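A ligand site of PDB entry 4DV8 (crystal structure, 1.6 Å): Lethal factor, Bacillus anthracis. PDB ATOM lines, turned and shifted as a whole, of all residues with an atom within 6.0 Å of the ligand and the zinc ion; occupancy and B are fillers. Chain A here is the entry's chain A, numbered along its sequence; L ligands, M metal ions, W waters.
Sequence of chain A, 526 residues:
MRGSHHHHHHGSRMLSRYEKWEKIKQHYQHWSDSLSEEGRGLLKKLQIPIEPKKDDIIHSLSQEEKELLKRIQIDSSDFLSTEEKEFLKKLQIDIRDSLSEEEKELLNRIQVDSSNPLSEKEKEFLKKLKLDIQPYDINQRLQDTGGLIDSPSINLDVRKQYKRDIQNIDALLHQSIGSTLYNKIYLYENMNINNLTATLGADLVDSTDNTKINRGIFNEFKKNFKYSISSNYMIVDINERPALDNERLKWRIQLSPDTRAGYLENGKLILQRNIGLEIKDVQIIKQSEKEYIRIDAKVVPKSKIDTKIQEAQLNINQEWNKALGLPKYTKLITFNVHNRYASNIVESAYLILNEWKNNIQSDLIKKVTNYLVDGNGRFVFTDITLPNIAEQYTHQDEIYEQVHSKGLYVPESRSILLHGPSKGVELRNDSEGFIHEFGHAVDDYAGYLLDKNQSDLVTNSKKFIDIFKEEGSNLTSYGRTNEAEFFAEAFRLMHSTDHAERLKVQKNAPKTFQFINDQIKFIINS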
ATOM      1  N   ASP A  78     -30.539  28.601  17.229  1.00  0.00           N
ATOM      2  CA  ASP A  78     -29.121  28.266  17.068  1.00  0.00           C
ATOM      3  C   ASP A  78     -28.683  28.153  15.604  1.00  0.00           C
ATOM      4  O   ASP A  78     -27.552  27.788  15.329  1.00  0.00           O
ATOM      5  CB  ASP A  78     -28.767  26.988  17.847  1.00  0.00           C
ATOM      6  CG  ASP A  78     -29.626  25.801  17.467  1.00  0.00           C
ATOM      7  OD1 ASP A  78     -30.114  25.761  16.321  1.00  0.00           O
ATOM      8  OD2 ASP A  78     -29.809  24.892  18.311  1.00  0.00           O
ATOM      9  N   PHE A  79     -29.569  28.519  14.673  1.00  0.00           N
ATOM     10  CA  PHE A  79     -29.330  28.242  13.251  1.00  0.00           C
ATOM     11  C   PHE A  79     -29.441  29.430  12.312  1.00  0.00           C
ATOM     12  O   PHE A  79     -29.214  29.291  11.102  1.00  0.00           O
ATOM     13  CB  PHE A  79     -30.289  27.151  12.780  1.00  0.00           C
ATOM     14  CG  PHE A  79     -31.731  27.457  13.056  1.00  0.00           C
ATOM     15  CD1 PHE A  79     -32.509  28.090  12.089  1.00  0.00           C
ATOM     16  CD2 PHE A  79     -32.311  27.131  14.262  1.00  0.00           C
ATOM     17  CE1 PHE A  79     -33.850  28.378  12.349  1.00  0.00           C
ATOM     18  CE2 PHE A  79     -33.641  27.414  14.527  1.00  0.00           C
ATOM     19  CZ  PHE A  79     -34.416  28.040  13.567  1.00  0.00           C
ATOM     20  N   GLU A 391     -19.447  20.548   2.200  1.00  0.00           N
ATOM     21  CA  GLU A 391     -19.530  19.494   3.213  1.00  0.00           C
ATOM     22  C   GLU A 391     -20.827  19.570   4.030  1.00  0.00           C
ATOM     23  O   GLU A 391     -21.238  18.562   4.616  1.00  0.00           O
ATOM     24  CB  GLU A 391     -18.276  19.500   4.120  1.00  0.00           C
ATOM     25  CG  GLU A 391     -17.016  18.981   3.452  1.00  0.00           C
ATOM     26  CD  GLU A 391     -16.322  19.997   2.549  1.00  0.00           C
ATOM     27  OE1 GLU A 391     -16.788  21.148   2.458  1.00  0.00           O
ATOM     28  OE2 GLU A 391     -15.295  19.632   1.918  1.00  0.00           O
ATOM     29  N   GLN A 392     -21.470  20.741   4.087  1.00  0.00           N
ATOM     30  CA  GLN A 392     -22.844  20.816   4.578  1.00  0.00           C
ATOM     31  C   GLN A 392     -23.908  20.681   3.482  1.00  0.00           C
ATOM     32  O   GLN A 392     -24.763  19.799   3.569  1.00  0.00           O
ATOM     33  CB  GLN A 392     -23.127  22.094   5.394  1.00  0.00           C
ATOM     34  CG  GLN A 392     -24.569  22.069   5.902  1.00  0.00           C
ATOM     35  CD  GLN A 392     -25.055  23.278   6.693  1.00  0.00           C
ATOM     36  OE1 GLN A 392     -26.143  23.230   7.265  1.00  0.00           O
ATOM     37  NE2 GLN A 392     -24.269  24.368   6.720  1.00  0.00           N
ATOM     38  N   GLN A 396     -27.490  18.553   3.205  1.00  0.00           N
ATOM     39  CA  GLN A 396     -28.719  19.224   3.604  1.00  0.00           C
ATOM     40  C   GLN A 396     -29.309  19.922   2.383  1.00  0.00           C
ATOM     41  O   GLN A 396     -29.046  21.115   2.168  1.00  0.00           O
ATOM     42  CB  GLN A 396     -28.443  20.251   4.715  1.00  0.00           C
ATOM     43  CG  GLN A 396     -27.568  19.753   5.873  1.00  0.00           C
ATOM     44  CD  GLN A 396     -28.318  18.882   6.873  1.00  0.00           C
ATOM     45  OE1 GLN A 396     -28.105  17.678   6.954  1.00  0.00           O
ATOM     46  NE2 GLN A 396     -29.185  19.508   7.663  1.00  0.00           N
ATOM     47  N   GLU A 401     -33.213  23.264   6.436  1.00  0.00           N
ATOM     48  CA  GLU A 401     -32.354  22.462   7.318  1.00  0.00           C
ATOM     49  C   GLU A 401     -30.882  22.912   7.316  1.00  0.00           C
ATOM     50  O   GLU A 401     -30.071  22.389   8.098  1.00  0.00           O
ATOM     51  CB  GLU A 401     -32.436  20.980   6.971  1.00  0.00           C
ATOM     52  CG  GLU A 401     -33.813  20.356   7.147  1.00  0.00           C
ATOM     53  CD  GLU A 401     -34.244  20.206   8.616  1.00  0.00           C
ATOM     54  OE1 GLU A 401     -35.281  19.563   8.836  1.00  0.00           O
ATOM     55  OE2 GLU A 401     -33.586  20.741   9.539  1.00  0.00           O
ATOM     56  N   GLN A 402     -30.544  23.851   6.440  1.00  0.00           N
ATOM     57  CA  GLN A 402     -29.189  24.391   6.415  1.00  0.00           C
ATOM     58  C   GLN A 402     -28.992  25.377   7.567  1.00  0.00           C
ATOM     59  O   GLN A 402     -29.927  26.098   7.976  1.00  0.00           O
ATOM     60  CB  GLN A 402     -28.910  25.062   5.064  1.00  0.00           C
ATOM     61  CG  GLN A 402     -28.912  24.079   3.910  1.00  0.00           C
ATOM     62  CD  GLN A 402     -28.807  24.781   2.583  1.00  0.00           C
ATOM     63  OE1 GLN A 402     -28.831  26.010   2.535  1.00  0.00           O
ATOM     64  NE2 GLN A 402     -28.724  24.007   1.498  1.00  0.00           N
ATOM     65  N   VAL A 403     -27.784  25.389   8.106  1.00  0.00           N
ATOM     66  CA  VAL A 403     -27.525  26.116   9.332  1.00  0.00           C
ATOM     67  C   VAL A 403     -26.357  27.084   9.211  1.00  0.00           C
ATOM     68  O   VAL A 403     -25.329  26.742   8.598  1.00  0.00           O
ATOM     69  CB  VAL A 403     -27.209  25.083  10.446  1.00  0.00           C
ATOM     70  CG1 VAL A 403     -26.647  25.754  11.670  1.00  0.00           C
ATOM     71  CG2 VAL A 403     -28.483  24.301  10.793  1.00  0.00           C
ATOM     72  N   HIS A 404     -26.470  28.299   9.725  1.00  0.00           N
ATOM     73  CA  HIS A 404     -25.235  29.033   9.964  1.00  0.00           C
ATOM     74  C   HIS A 404     -25.027  29.097  11.452  1.00  0.00           C
ATOM     75  O   HIS A 404     -25.974  29.284  12.232  1.00  0.00           O
ATOM     76  CB  HIS A 404     -25.176  30.422   9.303  1.00  0.00           C
ATOM     77  CG  HIS A 404     -23.836  31.094   9.419  1.00  0.00           C
ATOM     78  ND1 HIS A 404     -22.638  30.450   9.132  1.00  0.00           N
ATOM     79  CD2 HIS A 404     -23.499  32.345   9.792  1.00  0.00           C
ATOM     80  CE1 HIS A 404     -21.638  31.287   9.326  1.00  0.00           C
ATOM     81  NE2 HIS A 404     -22.127  32.448   9.731  1.00  0.00           N
ATOM     82  N   SER A 405     -23.781  28.915  11.830  1.00  0.00           N
ATOM     83  CA  SER A 405     -23.338  28.785  13.221  1.00  0.00           C
ATOM     84  C   SER A 405     -21.817  28.911  13.295  1.00  0.00           C
ATOM     85  O   SER A 405     -21.134  28.893  12.266  1.00  0.00           O
ATOM     86  CB  SER A 405     -23.768  27.430  13.791  1.00  0.00           C
ATOM     87  OG  SER A 405     -23.252  26.363  13.015  1.00  0.00           O
ATOM     88  N   LYS A 406     -21.278  29.007  14.513  1.00  0.00           N
ATOM     89  CA  LYS A 406     -19.838  29.109  14.685  1.00  0.00           C
ATOM     90  C   LYS A 406     -19.127  27.866  14.173  1.00  0.00           C
ATOM     91  O   LYS A 406     -18.037  27.948  13.576  1.00  0.00           O
ATOM     92  CB  LYS A 406     -19.505  29.338  16.168  1.00  0.00           C
ATOM     93  CG  LYS A 406     -18.001  29.318  16.486  1.00  0.00           C
ATOM     94  CD  LYS A 406     -17.304  30.478  15.769  1.00  0.00           C
ATOM     95  CE  LYS A 406     -15.806  30.342  15.898  1.00  0.00           C
ATOM     96  NZ  LYS A 406     -15.108  31.499  15.232  1.00  0.00           N
ATOM     97  N   GLY A 407     -19.730  26.711  14.400  1.00  0.00           N
ATOM     98  CA  GLY A 407     -19.177  25.458  13.913  1.00  0.00           C
ATOM     99  C   GLY A 407     -20.242  24.403  13.690  1.00  0.00           C
ATOM    100  O   GLY A 407     -21.377  24.553  14.134  1.00  0.00           O
ATOM    101  N   LEU A 408     -19.872  23.333  13.009  1.00  0.00           N
ATOM    102  CA  LEU A 408     -20.810  22.272  12.704  1.00  0.00           C
ATOM    103  C   LEU A 408     -20.058  20.953  12.598  1.00  0.00           C
ATOM    104  O   LEU A 408     -18.874  20.924  12.255  1.00  0.00           O
ATOM    105  CB  LEU A 408     -21.477  22.564  11.354  1.00  0.00           C
ATOM    106  CG  LEU A 408     -22.886  22.097  11.055  1.00  0.00           C
ATOM    107  CD1 LEU A 408     -23.890  22.530  12.124  1.00  0.00           C
ATOM    108  CD2 LEU A 408     -23.289  22.684   9.687  1.00  0.00           C
ATOM    109  N   TYR A 409     -20.753  19.862  12.865  1.00  0.00           N
ATOM    110  CA  TYR A 409     -20.257  18.542  12.512  1.00  0.00           C
ATOM    111  C   TYR A 409     -21.292  17.864  11.634  1.00  0.00           C
ATOM    112  O   TYR A 409     -22.444  17.709  12.041  1.00  0.00           O
ATOM    113  CB  TYR A 409     -19.943  17.676  13.753  1.00  0.00           C
ATOM    114  CG  TYR A 409     -19.534  16.268  13.339  1.00  0.00           C
ATOM    115  CD1 TYR A 409     -18.308  16.038  12.749  1.00  0.00           C
ATOM    116  CD2 TYR A 409     -20.411  15.195  13.473  1.00  0.00           C
ATOM    117  CE1 TYR A 409     -17.939  14.781  12.312  1.00  0.00           C
ATOM    118  CE2 TYR A 409     -20.048  13.916  13.047  1.00  0.00           C
ATOM    119  CZ  TYR A 409     -18.813  13.717  12.466  1.00  0.00           C
ATOM    120  OH  TYR A 409     -18.419  12.483  12.015  1.00  0.00           O
ATOM    121  N   VAL A 410     -20.874  17.478  10.428  1.00  0.00           N
ATOM    122  CA  VAL A 410     -21.780  16.839   9.492  1.00  0.00           C
ATOM    123  C   VAL A 410     -21.453  15.355   9.385  1.00  0.00           C
ATOM    124  O   VAL A 410     -20.474  14.971   8.765  1.00  0.00           O
ATOM    125  CB  VAL A 410     -21.672  17.471   8.092  1.00  0.00           C
ATOM    126  CG1 VAL A 410     -22.725  16.895   7.171  1.00  0.00           C
ATOM    127  CG2 VAL A 410     -21.819  18.991   8.189  1.00  0.00           C
ATOM    128  N   PRO A 411     -22.283  14.499  10.008  1.00  0.00           N
ATOM    129  CA  PRO A 411     -21.930  13.077  10.012  1.00  0.00           C
ATOM    130  C   PRO A 411     -21.850  12.497   8.610  1.00  0.00           C
ATOM    131  O   PRO A 411     -21.014  11.633   8.352  1.00  0.00           O
ATOM    132  CB  PRO A 411     -23.077  12.425  10.791  1.00  0.00           C
ATOM    133  CG  PRO A 411     -23.735  13.560  11.558  1.00  0.00           C
ATOM    134  CD  PRO A 411     -23.570  14.764  10.672  1.00  0.00           C
ATOM    135  N   GLU A 412     -22.694  12.976   7.694  1.00  0.00           N
ATOM    136  CA  GLU A 412     -22.729  12.423   6.348  1.00  0.00           C
ATOM    137  C   GLU A 412     -21.439  12.655   5.551  1.00  0.00           C
ATOM    138  O   GLU A 412     -21.128  11.886   4.631  1.00  0.00           O
ATOM    139  CB  GLU A 412     -23.930  12.956   5.569  1.00  0.00           C
ATOM    140  CG  GLU A 412     -25.294  12.529   6.105  1.00  0.00           C
ATOM    141  CD  GLU A 412     -25.855  13.452   7.187  1.00  0.00           C
ATOM    142  OE1 GLU A 412     -27.019  13.257   7.565  1.00  0.00           O
ATOM    143  OE2 GLU A 412     -25.129  14.352   7.673  1.00  0.00           O
ATOM    144  N   LEU A 418     -15.686  25.103  10.700  1.00  0.00           N
ATOM    145  CA  LEU A 418     -15.481  26.153  11.677  1.00  0.00           C
ATOM    146  C   LEU A 418     -15.434  27.502  10.987  1.00  0.00           C
ATOM    147  O   LEU A 418     -14.554  27.768  10.164  1.00  0.00           O
ATOM    148  CB  LEU A 418     -14.185  25.904  12.466  1.00  0.00           C
ATOM    149  CG  LEU A 418     -13.960  26.649  13.783  1.00  0.00           C
ATOM    150  CD1 LEU A 418     -14.948  26.189  14.836  1.00  0.00           C
ATOM    151  CD2 LEU A 418     -12.533  26.464  14.293  1.00  0.00           C
ATOM    152  N   GLY A 424     -19.132  32.188  19.013  1.00  0.00           N
ATOM    153  CA  GLY A 424     -20.124  31.414  19.738  1.00  0.00           C
ATOM    154  C   GLY A 424     -20.405  32.098  21.059  1.00  0.00           C
ATOM    155  O   GLY A 424     -19.479  32.539  21.744  1.00  0.00           O
ATOM    156  N   VAL A 425     -21.684  32.181  21.422  1.00  0.00           N
ATOM    157  CA  VAL A 425     -22.091  32.940  22.616  1.00  0.00           C
ATOM    158  C   VAL A 425     -21.406  32.489  23.921  1.00  0.00           C
ATOM    159  O   VAL A 425     -20.878  33.322  24.664  1.00  0.00           O
ATOM    160  CB  VAL A 425     -23.626  32.948  22.790  1.00  0.00           C
ATOM    161  CG1 VAL A 425     -24.021  33.915  23.901  1.00  0.00           C
ATOM    162  CG2 VAL A 425     -24.304  33.343  21.489  1.00  0.00           C
ATOM    163  N   GLU A 426     -21.410  31.190  24.199  1.00  0.00           N
ATOM    164  CA  GLU A 426     -20.806  30.695  25.439  1.00  0.00           C
ATOM    165  C   GLU A 426     -19.379  30.178  25.231  1.00  0.00           C
ATOM    166  O   GLU A 426     -18.873  29.408  26.055  1.00  0.00           O
ATOM    167  CB  GLU A 426     -21.670  29.600  26.072  1.00  0.00           C
ATOM    168  CG  GLU A 426     -23.038  30.064  26.593  1.00  0.00           C
ATOM    169  CD  GLU A 426     -23.848  28.933  27.220  1.00  0.00           C
ATOM    170  OE1 GLU A 426     -24.499  28.169  26.465  1.00  0.00           O
ATOM    171  OE2 GLU A 426     -23.839  28.816  28.455  1.00  0.00           O
ATOM    172  N   LEU A 427     -18.731  30.602  24.154  1.00  0.00           N
ATOM    173  CA  LEU A 427     -17.374  30.161  23.843  1.00  0.00           C
ATOM    174  C   LEU A 427     -16.404  31.334  23.912  1.00  0.00           C
ATOM    175  O   LEU A 427     -16.693  32.415  23.403  1.00  0.00           O
ATOM    176  CB  LEU A 427     -17.302  29.544  22.439  1.00  0.00           C
ATOM    177  CG  LEU A 427     -18.198  28.370  22.080  1.00  0.00           C
ATOM    178  CD1 LEU A 427     -18.091  28.051  20.594  1.00  0.00           C
ATOM    179  CD2 LEU A 427     -17.850  27.144  22.905  1.00  0.00           C
ATOM    180  N   GLY A 433     -14.793  26.061  20.159  1.00  0.00           N
ATOM    181  CA  GLY A 433     -15.743  25.675  19.139  1.00  0.00           C
ATOM    182  C   GLY A 433     -15.310  24.416  18.415  1.00  0.00           C
ATOM    183  O   GLY A 433     -16.131  23.531  18.170  1.00  0.00           O
ATOM    184  N   PHE A 434     -14.030  24.326  18.059  1.00  0.00           N
ATOM    185  CA  PHE A 434     -13.544  23.152  17.338  1.00  0.00           C
ATOM    186  C   PHE A 434     -13.686  21.915  18.215  1.00  0.00           C
ATOM    187  O   PHE A 434     -14.064  20.843  17.737  1.00  0.00           O
ATOM    188  CB  PHE A 434     -12.091  23.342  16.911  1.00  0.00           C
ATOM    189  CG  PHE A 434     -11.582  22.230  16.033  1.00  0.00           C
ATOM    190  CD1 PHE A 434     -11.785  22.262  14.664  1.00  0.00           C
ATOM    191  CD2 PHE A 434     -10.915  21.134  16.579  1.00  0.00           C
ATOM    192  CE1 PHE A 434     -11.324  21.234  13.845  1.00  0.00           C
ATOM    193  CE2 PHE A 434     -10.461  20.106  15.775  1.00  0.00           C
ATOM    194  CZ  PHE A 434     -10.656  20.154  14.403  1.00  0.00           C
ATOM    195  N   HIS A 436     -15.809  21.429  20.673  1.00  0.00           N
ATOM    196  CA  HIS A 436     -17.214  21.086  20.650  1.00  0.00           C
ATOM    197  C   HIS A 436     -17.559  20.213  19.435  1.00  0.00           C
ATOM    198  O   HIS A 436     -18.191  19.169  19.576  1.00  0.00           O
ATOM    199  CB  HIS A 436     -18.054  22.372  20.661  1.00  0.00           C
ATOM    200  CG  HIS A 436     -19.521  22.127  20.538  1.00  0.00           C
ATOM    201  ND1 HIS A 436     -20.369  22.088  21.635  1.00  0.00           N
ATOM    202  CD2 HIS A 436     -20.308  21.934  19.459  1.00  0.00           C
ATOM    203  CE1 HIS A 436     -21.598  21.863  21.232  1.00  0.00           C
ATOM    204  NE2 HIS A 436     -21.594  21.766  19.908  1.00  0.00           N
ATOM    205  N   GLU A 437     -17.130  20.614  18.229  1.00  0.00           N
ATOM    206  CA  GLU A 437     -17.442  19.806  17.058  1.00  0.00           C
ATOM    207  C   GLU A 437     -16.783  18.441  17.127  1.00  0.00           C
ATOM    208  O   GLU A 437     -17.388  17.459  16.684  1.00  0.00           O
ATOM    209  CB  GLU A 437     -17.054  20.501  15.749  1.00  0.00           C
ATOM    210  CG  GLU A 437     -17.540  21.939  15.609  1.00  0.00           C
ATOM    211  CD  GLU A 437     -18.999  22.107  15.882  1.00  0.00           C
ATOM    212  OE1 GLU A 437     -19.391  23.233  16.243  1.00  0.00           O
ATOM    213  OE2 GLU A 437     -19.785  21.130  15.764  1.00  0.00           O
ATOM    214  N   HIS A 440     -18.879  15.970  18.814  1.00  0.00           N
ATOM    215  CA  HIS A 440     -19.849  15.310  17.958  1.00  0.00           C
ATOM    216  C   HIS A 440     -19.234  14.153  17.173  1.00  0.00           C
ATOM    217  O   HIS A 440     -19.879  13.128  16.960  1.00  0.00           O
ATOM    218  CB  HIS A 440     -20.416  16.292  16.942  1.00  0.00           C
ATOM    219  CG  HIS A 440     -21.405  17.272  17.515  1.00  0.00           C
ATOM    220  ND1 HIS A 440     -22.458  16.888  18.290  1.00  0.00           N
ATOM    221  CD2 HIS A 440     -21.483  18.615  17.364  1.00  0.00           C
ATOM    222  CE1 HIS A 440     -23.168  17.966  18.624  1.00  0.00           C
ATOM    223  NE2 HIS A 440     -22.600  19.003  18.068  1.00  0.00           N
ATOM    224  N   TYR A 478     -26.656  26.065  26.394  1.00  0.00           N
ATOM    225  CA  TYR A 478     -26.764  25.470  25.073  1.00  0.00           C
ATOM    226  C   TYR A 478     -26.801  23.936  25.166  1.00  0.00           C
ATOM    227  O   TYR A 478     -27.453  23.268  24.357  1.00  0.00           O
ATOM    228  CB  TYR A 478     -25.666  25.958  24.119  1.00  0.00           C
ATOM    229  CG  TYR A 478     -25.787  25.316  22.763  1.00  0.00           C
ATOM    230  CD1 TYR A 478     -26.920  25.514  21.992  1.00  0.00           C
ATOM    231  CD2 TYR A 478     -24.795  24.487  22.275  1.00  0.00           C
ATOM    232  CE1 TYR A 478     -27.061  24.915  20.758  1.00  0.00           C
ATOM    233  CE2 TYR A 478     -24.919  23.888  21.023  1.00  0.00           C
ATOM    234  CZ  TYR A 478     -26.069  24.102  20.282  1.00  0.00           C
ATOM    235  OH  TYR A 478     -26.234  23.494  19.076  1.00  0.00           O
ATOM    236  N   ALA A 484     -27.334  15.253  21.848  1.00  0.00           N
ATOM    237  CA  ALA A 484     -26.086  15.414  21.110  1.00  0.00           C
ATOM    238  C   ALA A 484     -25.345  16.662  21.549  1.00  0.00           C
ATOM    239  O   ALA A 484     -24.130  16.636  21.706  1.00  0.00           O
ATOM    240  CB  ALA A 484     -26.359  15.447  19.602  1.00  0.00           C
ATOM    241  N   GLU A 485     -26.071  17.761  21.717  1.00  0.00           N
ATOM    242  CA  GLU A 485     -25.419  18.995  22.117  1.00  0.00           C
ATOM    243  C   GLU A 485     -24.903  18.934  23.544  1.00  0.00           C
ATOM    244  O   GLU A 485     -23.841  19.466  23.838  1.00  0.00           O
ATOM    245  CB  GLU A 485     -26.347  20.198  21.951  1.00  0.00           C
ATOM    246  CG  GLU A 485     -26.839  20.389  20.505  1.00  0.00           C
ATOM    247  CD  GLU A 485     -25.717  20.440  19.499  1.00  0.00           C
ATOM    248  OE1 GLU A 485     -24.571  20.755  19.894  1.00  0.00           O
ATOM    249  OE2 GLU A 485     -25.978  20.180  18.303  1.00  0.00           O
ATOM    250  N   ALA A 488     -21.668  16.996  23.477  1.00  0.00           N
ATOM    251  CA  ALA A 488     -20.599  17.784  22.888  1.00  0.00           C
ATOM    252  C   ALA A 488     -20.127  18.870  23.831  1.00  0.00           C
ATOM    253  O   ALA A 488     -18.925  19.153  23.929  1.00  0.00           O
ATOM    254  CB  ALA A 488     -21.052  18.395  21.541  1.00  0.00           C
ATOM    255  N   GLU A 489     -21.077  19.467  24.553  1.00  0.00           N
ATOM    256  CA  GLU A 489     -20.758  20.501  25.524  1.00  0.00           C
ATOM    257  C   GLU A 489     -20.009  19.913  26.724  1.00  0.00           C
ATOM    258  O   GLU A 489     -19.002  20.472  27.163  1.00  0.00           O
ATOM    259  CB  GLU A 489     -22.033  21.222  25.978  1.00  0.00           C
ATOM    260  CG  GLU A 489     -22.523  22.287  24.981  1.00  0.00           C
ATOM    261  CD  GLU A 489     -21.558  23.452  24.871  1.00  0.00           C
ATOM    262  OE1 GLU A 489     -21.745  24.441  25.605  1.00  0.00           O
ATOM    263  OE2 GLU A 489     -20.601  23.359  24.086  1.00  0.00           O
ATOM    264  N   ARG A 492     -16.541  19.162  25.550  1.00  0.00           N
ATOM    265  CA  ARG A 492     -15.717  20.366  25.420  1.00  0.00           C
ATOM    266  C   ARG A 492     -15.224  20.860  26.770  1.00  0.00           C
ATOM    267  O   ARG A 492     -14.040  21.182  26.947  1.00  0.00           O
ATOM    268  CB  ARG A 492     -16.486  21.469  24.683  1.00  0.00           C
ATOM    269  CG  ARG A 492     -15.977  22.859  25.014  1.00  0.00           C
ATOM    270  CD  ARG A 492     -16.787  23.936  24.361  1.00  0.00           C
ATOM    271  NE  ARG A 492     -18.058  24.267  25.036  1.00  0.00           N
ATOM    272  CZ  ARG A 492     -18.189  25.209  25.967  1.00  0.00           C
ATOM    273  NH1 ARG A 492     -17.124  25.888  26.397  1.00  0.00           N
ATOM    274  NH2 ARG A 492     -19.371  25.467  26.489  1.00  0.00           N
HETATM  275  O1  LIG L   1     -23.918  23.039  17.979  1.00  0.00           O
HETATM  276  C1  LIG L   1     -23.400  23.565  17.024  1.00  0.00           C
HETATM  277  N1  LIG L   1     -22.383  22.905  16.296  1.00  0.00           N
HETATM  278  O2  LIG L   1     -22.114  21.623  16.562  1.00  0.00           O
HETATM  279  C2  LIG L   1     -23.767  24.980  16.698  1.00  0.00           C
HETATM  280  C3  LIG L   1     -25.194  25.101  16.361  1.00  0.00           C
HETATM  281  C4  LIG L   1     -25.509  24.345  15.048  1.00  0.00           C
HETATM  282  C5  LIG L   1     -26.834  23.627  15.129  1.00  0.00           C
HETATM  283  C6  LIG L   1     -27.035  22.607  13.989  1.00  0.00           C
HETATM  284  N2  LIG L   1     -27.305  21.240  14.528  1.00  0.00           N
HETATM  285  C7  LIG L   1     -27.986  20.425  13.553  1.00  0.00           C
HETATM  286  C8  LIG L   1     -27.208  20.243  12.306  1.00  0.00           C
HETATM  287  C9  LIG L   1     -26.033  19.461  12.284  1.00  0.00           C
HETATM  288  C10 LIG L   1     -25.299  19.307  11.086  1.00  0.00           C
HETATM  289  C11 LIG L   1     -25.767  19.917   9.916  1.00  0.00           C
HETATM  290  C12 LIG L   1     -26.942  20.691   9.931  1.00  0.00           C
HETATM  291  C13 LIG L   1     -27.667  20.847  11.128  1.00  0.00           C
HETATM  292  F1  LIG L   1     -25.108  19.800   8.772  1.00  0.00           F
HETATM  293  C14 LIG L   1     -23.381  25.865  17.925  1.00  0.00           C
HETATM  294  C15 LIG L   1     -21.954  25.646  18.367  1.00  0.00           C
HETATM  295  O3  LIG L   1     -21.016  26.165  17.498  1.00  0.00           O
HETATM  296  C16 LIG L   1     -19.670  25.979  17.763  1.00  0.00           C
HETATM  297  C17 LIG L   1     -21.745  26.306  19.711  1.00  0.00           C
HETATM  298  C18 LIG L   1     -21.427  25.507  20.807  1.00  0.00           C
HETATM  299  C19 LIG L   1     -21.269  26.067  22.056  1.00  0.00           C
HETATM  300  C20 LIG L   1     -21.447  27.447  22.233  1.00  0.00           C
HETATM  301  C21 LIG L   1     -21.755  28.262  21.147  1.00  0.00           C
HETATM  302  C22 LIG L   1     -21.916  27.693  19.878  1.00  0.00           C
HETATM  303  F2  LIG L   1     -21.301  27.967  23.452  1.00  0.00           F
HETATM  304 ZN    ZN M   1     -23.065  21.058  18.438  1.00  0.00          ZN
HETATM  305  O   HOH W   1     -26.247  16.562   8.791  1.00  0.00           O
HETATM  306  O   HOH W   2     -23.108  20.150  14.582  1.00  0.00           O
HETATM  307  O   HOH W   3     -24.278  29.470  23.856  1.00  0.00           O
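OE1 of Glu 437 sits at hydrogen-bond distance from N1 of the ligand, at 3.0 Å. O1 of the ligand lies close to OH of Tyr 478 (2.6 Å). N of Gly 407 lies within hydrogen-bond range of O3 of the ligand, at 3.4 Å. O of Gly 407 lies within hydrogen-bond range of N1 of the ligand, 2.9 Å away.
The side-chain carboxylate (OE2) of Glu 489 sits at hydrogen-bond distance from a ring nitrogen (ND1) of His 436 (2.8 Å). OE2 of Glu 437 sits at hydrogen-bond distance from N of Tyr 409 (3.3 Å). The side-chain carboxylate of Glu 437 sits close to the backbone NH of Leu 408. The backbone carbonyl oxygen (O) of Gly 407 sits at hydrogen-bond distance from the side-chain hydroxyl (OG) of Ser 405 (2.8 Å). The side-chain amide nitrogen (NE2) of Gln 396 sits at hydrogen-bond distance from the backbone carbonyl oxygen (O) of Glu 401 (3.0 Å). O of Gln 396 sits at hydrogen-bond distance from NE2 of Gln 402, at 3.0 Å. OE1 of Glu 489 is in salt-bridge range of NH2 of Arg 492 (2.7 Å). The backbone NH (N) of Val 403 is in hydrogen-bond range of the side-chain amide oxygen (OE1) of Gln 392 (2.8 Å).
N of Glu 426 lies close to F2 of the ligand, 3.3 Å away. Asp 78 touches the ligand. Gln 392 touches the ligand (CG to F1, 3.7 Å). Gln 396 touches the ligand (NE2 to C12, 3.4 Å). Val 403 touches the ligand (CG2 to C13, 3.6 Å). Ser 405 touches the ligand. CB of Lys 406 touches C16 of the ligand, 3.7 Å away. Leu 408 touches the ligand (CD2 to F1, 3.5 Å). O of Tyr 409 touches C10 of the ligand, 3.4 Å away. Val 410 touches the ligand (CG2 to F1, 3.4 Å). Gly 424 touches the ligand. N of Val 425 touches C21 of the ligand (3.9 Å). Leu 427 touches the ligand (CG to C20, 3.4 Å). OE2 of Glu 489 touches C19 of the ligand, at 3.4 Å. Hydrophobic or aromatic side chains that line the ligand: Val 403, Leu 408, Val 410, Leu 427, His 436, His 440 and Tyr 478. 20 residues have an atom within 4 Å of the ligand: Asp 78, Gln 392, Gln 396, Val 403, Ser 405, Lys 406, Gly 407, Leu 408, Tyr 409, Val 410, Gly 424, Val 425, Glu 426, Leu 427, His 436, Glu 437, His 440, Tyr 478, Glu 485 and Glu 489. The nearest printed residue that does not touch the ligand is Glu 401 (4.004 Å).
Within 4 Å of the zinc ion: His 436, His 440 and Glu 485. The nearest printed residue that does not touch the zinc ion is Tyr 478 (4.05 Å).
The zinc ion is bound by the side-chain carboxylate (OE1) of Glu 485 (2.1 Å), a ring nitrogen (NE2) of His 440 (2.1 Å), an oxygen (O2) of the ligand (2.2 Å), a ring nitrogen (NE2) of His 436 (2.2 Å) and an oxygen (O1) of the ligand (2.2 Å).
Water W2 bridges N of Tyr 409 and N1 of the ligand. Water W1 bridges OE2 of Glu 412 (2.7 Å) and OE1 of Gln 396 (2.8 Å).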
